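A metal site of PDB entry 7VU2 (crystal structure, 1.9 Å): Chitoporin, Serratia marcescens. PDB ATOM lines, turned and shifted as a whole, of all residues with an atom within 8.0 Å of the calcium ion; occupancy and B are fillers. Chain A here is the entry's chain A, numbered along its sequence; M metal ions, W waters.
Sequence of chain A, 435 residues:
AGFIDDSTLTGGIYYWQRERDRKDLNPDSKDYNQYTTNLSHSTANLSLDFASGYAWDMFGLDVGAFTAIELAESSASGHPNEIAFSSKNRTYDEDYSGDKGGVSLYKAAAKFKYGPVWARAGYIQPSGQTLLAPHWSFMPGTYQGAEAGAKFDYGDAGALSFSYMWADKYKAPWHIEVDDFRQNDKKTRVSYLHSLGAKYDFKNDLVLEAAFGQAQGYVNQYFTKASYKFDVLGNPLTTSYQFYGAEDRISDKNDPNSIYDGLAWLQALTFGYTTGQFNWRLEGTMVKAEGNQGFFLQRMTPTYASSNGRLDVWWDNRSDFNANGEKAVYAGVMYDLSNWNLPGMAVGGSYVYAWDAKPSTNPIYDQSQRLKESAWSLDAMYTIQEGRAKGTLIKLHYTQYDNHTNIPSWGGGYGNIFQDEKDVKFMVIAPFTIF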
ATOM      1  N   TYR A 218      -4.426   9.420   7.942  1.00  0.00           N
ATOM      2  CA  TYR A 218      -4.481  10.870   7.923  1.00  0.00           C
ATOM      3  C   TYR A 218      -3.718  11.579   6.819  1.00  0.00           C
ATOM      4  O   TYR A 218      -4.306  12.436   6.158  1.00  0.00           O
ATOM      5  CB  TYR A 218      -3.989  11.384   9.286  1.00  0.00           C
ATOM      6  CG  TYR A 218      -4.286  12.817   9.599  1.00  0.00           C
ATOM      7  CD1 TYR A 218      -5.555  13.346   9.392  1.00  0.00           C
ATOM      8  CD2 TYR A 218      -3.312  13.646  10.122  1.00  0.00           C
ATOM      9  CE1 TYR A 218      -5.840  14.663   9.687  1.00  0.00           C
ATOM     10  CE2 TYR A 218      -3.591  14.964  10.436  1.00  0.00           C
ATOM     11  CZ  TYR A 218      -4.843  15.470  10.203  1.00  0.00           C
ATOM     12  OH  TYR A 218      -5.113  16.785  10.514  1.00  0.00           O
ATOM     13  N   GLU A 247      -0.830  15.025   0.960  1.00  0.00           N
ATOM     14  CA  GLU A 247      -2.282  15.043   0.843  1.00  0.00           C
ATOM     15  C   GLU A 247      -2.794  14.512   2.165  1.00  0.00           C
ATOM     16  O   GLU A 247      -2.124  13.711   2.825  1.00  0.00           O
ATOM     17  CB  GLU A 247      -2.755  14.209  -0.345  1.00  0.00           C
ATOM     18  CG  GLU A 247      -2.307  12.758  -0.306  1.00  0.00           C
ATOM     19  CD  GLU A 247      -2.505  12.055  -1.631  1.00  0.00           C
ATOM     20  OE1 GLU A 247      -2.977  12.699  -2.594  1.00  0.00           O
ATOM     21  OE2 GLU A 247      -2.200  10.838  -1.717  1.00  0.00           O
ATOM     22  N   ASP A 248      -3.958  14.976   2.585  1.00  0.00           N
ATOM     23  CA  ASP A 248      -4.587  14.333   3.733  1.00  0.00           C
ATOM     24  C   ASP A 248      -5.657  13.380   3.221  1.00  0.00           C
ATOM     25  O   ASP A 248      -5.919  13.269   2.025  1.00  0.00           O
ATOM     26  CB  ASP A 248      -5.108  15.370   4.736  1.00  0.00           C
ATOM     27  CG  ASP A 248      -6.315  16.136   4.258  1.00  0.00           C
ATOM     28  OD1 ASP A 248      -7.113  15.608   3.449  1.00  0.00           O
ATOM     29  OD2 ASP A 248      -6.484  17.272   4.736  1.00  0.00           O
ATOM     30  N   ARG A 249      -6.243  12.625   4.160  1.00  0.00           N
ATOM     31  CA  ARG A 249      -7.288  11.654   3.820  1.00  0.00           C
ATOM     32  C   ARG A 249      -8.644  12.075   4.374  1.00  0.00           C
ATOM     33  O   ARG A 249      -9.484  11.232   4.676  1.00  0.00           O
ATOM     34  CB  ARG A 249      -6.881  10.281   4.336  1.00  0.00           C
ATOM     35  CG  ARG A 249      -5.490   9.924   3.840  1.00  0.00           C
ATOM     36  CD  ARG A 249      -5.074   8.576   4.277  1.00  0.00           C
ATOM     37  NE  ARG A 249      -5.906   7.533   3.708  1.00  0.00           N
ATOM     38  CZ  ARG A 249      -5.712   6.252   3.964  1.00  0.00           C
ATOM     39  NH1 ARG A 249      -4.690   5.909   4.743  1.00  0.00           N
ATOM     40  NH2 ARG A 249      -6.497   5.333   3.444  1.00  0.00           N
ATOM     41  N   ILE A 250      -8.853  13.382   4.494  1.00  0.00           N
ATOM     42  CA  ILE A 250     -10.144  13.970   4.918  1.00  0.00           C
ATOM     43  C   ILE A 250     -10.553  14.919   3.806  1.00  0.00           C
ATOM     44  O   ILE A 250     -10.140  16.080   3.759  1.00  0.00           O
ATOM     45  CB  ILE A 250     -10.040  14.710   6.253  1.00  0.00           C
ATOM     46  CG1 ILE A 250      -9.548  13.736   7.339  1.00  0.00           C
ATOM     47  CG2 ILE A 250     -11.380  15.347   6.669  1.00  0.00           C
ATOM     48  CD1 ILE A 250      -9.394  14.328   8.677  1.00  0.00           C
ATOM     49  N   SER A 251     -11.409  14.436   2.898  1.00  0.00           N
ATOM     50  CA  SER A 251     -11.789  15.210   1.723  1.00  0.00           C
ATOM     51  C   SER A 251     -12.618  16.445   2.066  1.00  0.00           C
ATOM     52  O   SER A 251     -12.548  17.447   1.345  1.00  0.00           O
ATOM     53  CB  SER A 251     -12.596  14.337   0.751  1.00  0.00           C
ATOM     54  OG  SER A 251     -11.888  13.148   0.468  1.00  0.00           O
ATOM     55  N   ASP A 252     -13.435  16.376   3.124  1.00  0.00           N
ATOM     56  CA  ASP A 252     -14.327  17.468   3.499  1.00  0.00           C
ATOM     57  C   ASP A 252     -13.506  18.670   3.923  1.00  0.00           C
ATOM     58  O   ASP A 252     -12.902  18.684   5.005  1.00  0.00           O
ATOM     59  CB  ASP A 252     -15.272  17.035   4.617  1.00  0.00           C
ATOM     60  CG  ASP A 252     -16.247  18.135   5.042  1.00  0.00           C
ATOM     61  OD1 ASP A 252     -16.321  19.212   4.376  1.00  0.00           O
ATOM     62  OD2 ASP A 252     -16.940  17.922   6.045  1.00  0.00           O
ATOM     63  N   LYS A 253     -13.505  19.706   3.085  1.00  0.00           N
ATOM     64  CA  LYS A 253     -12.569  20.805   3.263  1.00  0.00           C
ATOM     65  C   LYS A 253     -12.835  21.614   4.521  1.00  0.00           C
ATOM     66  O   LYS A 253     -11.922  22.248   5.048  1.00  0.00           O
ATOM     67  CB  LYS A 253     -12.601  21.697   2.021  1.00  0.00           C
ATOM     68  CG  LYS A 253     -13.877  22.496   1.851  1.00  0.00           C
ATOM     69  CD  LYS A 253     -13.748  23.601   0.783  1.00  0.00           C
ATOM     70  CE  LYS A 253     -13.126  23.118  -0.518  1.00  0.00           C
ATOM     71  NZ  LYS A 253     -13.923  22.026  -1.160  1.00  0.00           N
ATOM     72  N   ASN A 254     -14.065  21.622   5.039  1.00  0.00           N
ATOM     73  CA  ASN A 254     -14.344  22.382   6.252  1.00  0.00           C
ATOM     74  C   ASN A 254     -14.295  21.520   7.507  1.00  0.00           C
ATOM     75  O   ASN A 254     -14.599  22.027   8.598  1.00  0.00           O
ATOM     76  CB  ASN A 254     -15.704  23.082   6.129  1.00  0.00           C
ATOM     77  CG  ASN A 254     -15.754  24.060   4.963  1.00  0.00           C
ATOM     78  OD1 ASN A 254     -14.799  24.816   4.712  1.00  0.00           O
ATOM     79  ND2 ASN A 254     -16.856  24.044   4.247  1.00  0.00           N
ATOM     80  N   ASP A 255     -13.901  20.265   7.392  1.00  0.00           N
ATOM     81  CA  ASP A 255     -13.596  19.453   8.564  1.00  0.00           C
ATOM     82  C   ASP A 255     -12.398  20.061   9.268  1.00  0.00           C
ATOM     83  O   ASP A 255     -11.394  20.400   8.604  1.00  0.00           O
ATOM     84  CB  ASP A 255     -13.305  18.010   8.138  1.00  0.00           C
ATOM     85  CG  ASP A 255     -13.160  17.054   9.322  1.00  0.00           C
ATOM     86  OD1 ASP A 255     -12.323  17.293  10.222  1.00  0.00           O
ATOM     87  OD2 ASP A 255     -13.854  16.033   9.330  1.00  0.00           O
ATOM     88  N   ASN A 257     -10.096  18.790  10.938  1.00  0.00           N
ATOM     89  CA  ASN A 257      -8.893  17.994  10.772  1.00  0.00           C
ATOM     90  C   ASN A 257      -8.405  17.934   9.329  1.00  0.00           C
ATOM     91  O   ASN A 257      -7.330  17.390   9.095  1.00  0.00           O
ATOM     92  CB  ASN A 257      -9.121  16.589  11.301  1.00  0.00           C
ATOM     93  CG  ASN A 257      -9.106  16.546  12.787  1.00  0.00           C
ATOM     94  OD1 ASN A 257      -8.129  16.962  13.423  1.00  0.00           O
ATOM     95  ND2 ASN A 257     -10.190  16.058  13.372  1.00  0.00           N
ATOM     96  N   SER A 258      -9.145  18.506   8.370  1.00  0.00           N
ATOM     97  CA  SER A 258      -8.636  18.640   7.013  1.00  0.00           C
ATOM     98  C   SER A 258      -7.619  19.779   7.000  1.00  0.00           C
ATOM     99  O   SER A 258      -7.934  20.888   7.448  1.00  0.00           O
ATOM    100  CB  SER A 258      -9.753  18.953   6.014  1.00  0.00           C
ATOM    101  OG  SER A 258      -9.205  19.205   4.719  1.00  0.00           O
ATOM    102  N   ILE A 259      -6.408  19.492   6.520  1.00  0.00           N
ATOM    103  CA  ILE A 259      -5.370  20.500   6.434  1.00  0.00           C
ATOM    104  C   ILE A 259      -5.014  20.860   4.998  1.00  0.00           C
ATOM    105  O   ILE A 259      -4.593  21.987   4.739  1.00  0.00           O
ATOM    106  CB  ILE A 259      -4.113  20.069   7.212  1.00  0.00           C
ATOM    107  CG1 ILE A 259      -3.618  18.680   6.784  1.00  0.00           C
ATOM    108  CG2 ILE A 259      -4.399  20.117   8.701  1.00  0.00           C
ATOM    109  CD1 ILE A 259      -2.291  18.315   7.480  1.00  0.00           C
ATOM    110  N   TYR A 260      -5.198  19.935   4.054  1.00  0.00           N
ATOM    111  CA  TYR A 260      -4.934  20.186   2.658  1.00  0.00           C
ATOM    112  C   TYR A 260      -6.168  19.879   1.818  1.00  0.00           C
ATOM    113  O   TYR A 260      -6.953  18.980   2.157  1.00  0.00           O
ATOM    114  CB  TYR A 260      -3.799  19.328   2.117  1.00  0.00           C
ATOM    115  CG  TYR A 260      -2.487  19.413   2.861  1.00  0.00           C
ATOM    116  CD1 TYR A 260      -1.777  20.605   2.920  1.00  0.00           C
ATOM    117  CD2 TYR A 260      -1.932  18.295   3.456  1.00  0.00           C
ATOM    118  CE1 TYR A 260      -0.565  20.695   3.560  1.00  0.00           C
ATOM    119  CE2 TYR A 260      -0.699  18.361   4.122  1.00  0.00           C
ATOM    120  CZ  TYR A 260      -0.034  19.566   4.164  1.00  0.00           C
ATOM    121  OH  TYR A 260       1.176  19.678   4.803  1.00  0.00           O
ATOM    122  N   ASP A 261      -6.320  20.604   0.715  1.00  0.00           N
ATOM    123  CA  ASP A 261      -7.291  20.290  -0.323  1.00  0.00           C
ATOM    124  C   ASP A 261      -6.525  19.791  -1.546  1.00  0.00           C
ATOM    125  O   ASP A 261      -5.722  20.548  -2.126  1.00  0.00           O
ATOM    126  CB  ASP A 261      -8.145  21.494  -0.723  1.00  0.00           C
ATOM    127  CG  ASP A 261      -9.007  21.998   0.405  1.00  0.00           C
ATOM    128  OD1 ASP A 261      -9.141  21.328   1.467  1.00  0.00           O
ATOM    129  OD2 ASP A 261      -9.548  23.107   0.221  1.00  0.00           O
ATOM    130  N   GLY A 262      -6.774  18.546  -1.934  1.00  0.00           N
ATOM    131  CA  GLY A 262      -5.991  17.934  -2.985  1.00  0.00           C
ATOM    132  C   GLY A 262      -4.532  17.829  -2.588  1.00  0.00           C
ATOM    133  O   GLY A 262      -4.173  17.782  -1.404  1.00  0.00           O
ATOM    134  N   GLU A 290      -3.405  24.580  -0.898  1.00  0.00           N
ATOM    135  CA  GLU A 290      -4.808  24.845  -0.667  1.00  0.00           C
ATOM    136  C   GLU A 290      -5.300  24.018   0.520  1.00  0.00           C
ATOM    137  O   GLU A 290      -4.704  22.988   0.872  1.00  0.00           O
ATOM    138  CB  GLU A 290      -5.610  24.541  -1.936  1.00  0.00           C
ATOM    139  CG  GLU A 290      -5.219  25.454  -3.094  1.00  0.00           C
ATOM    140  CD  GLU A 290      -6.033  25.221  -4.353  1.00  0.00           C
ATOM    141  OE1 GLU A 290      -6.842  24.278  -4.384  1.00  0.00           O
ATOM    142  OE2 GLU A 290      -5.849  25.990  -5.321  1.00  0.00           O
ATOM    143  N   GLY A 291      -6.370  24.489   1.151  1.00  0.00           N
ATOM    144  CA  GLY A 291      -6.914  23.842   2.323  1.00  0.00           C
ATOM    145  C   GLY A 291      -6.839  24.724   3.552  1.00  0.00           C
ATOM    146  O   GLY A 291      -6.396  25.866   3.518  1.00  0.00           O
ATOM    147  N   ASN A 292      -7.290  24.141   4.676  1.00  0.00           N
ATOM    148  CA  ASN A 292      -7.416  24.933   5.897  1.00  0.00           C
ATOM    149  C   ASN A 292      -6.051  25.443   6.369  1.00  0.00           C
ATOM    150  O   ASN A 292      -5.954  26.546   6.906  1.00  0.00           O
ATOM    151  CB  ASN A 292      -8.064  24.102   6.991  1.00  0.00           C
ATOM    152  CG  ASN A 292      -9.556  23.970   6.814  1.00  0.00           C
ATOM    153  OD1 ASN A 292     -10.208  24.876   6.278  1.00  0.00           O
ATOM    154  ND2 ASN A 292     -10.106  22.833   7.215  1.00  0.00           N
HETATM  155 CA    CA M   1      -8.412  17.552   3.101  1.00  0.00          CA
HETATM  156  O   HOH W   1      -8.330  16.337   0.936  1.00  0.00           O
HETATM  157  O   HOH W   2      -9.999  18.862   1.655  1.00  0.00           O
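O of Ser 258 sits at hydrogen-bond distance from ND2 of Asn 292. The side-chain carboxylate of Asp 248 lies close to the backbone NH of Ile 259 (2.8 Å).
The nearest printed residue that does not touch the calcium ion is Asp 261 (4.2 Å).
O of Tyr 260 binds the calcium ion, 2.2 Å away. The backbone carbonyl oxygen (O) of Ile 250 binds the calcium ion (2.4 Å). The calcium ion is bound by the side-chain carboxylate (OD1) of Asp 248, 2.4 Å away. The calcium ion is bound by OG of Ser 258, at 2.4 Å. Water W1 binds the calcium ion, 2.5 Å away. The calcium ion is bound by water W2 (2.5 Å). The calcium ion is bound by OD2 of Asp 248, at 2.5 Å.
Water W2 lies within hydrogen-bond range of the side-chain carboxylate (OD1) of Asp 261 (2.6 Å) and the backbone carbonyl oxygen (O) of Ser 251 (2.9 Å).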
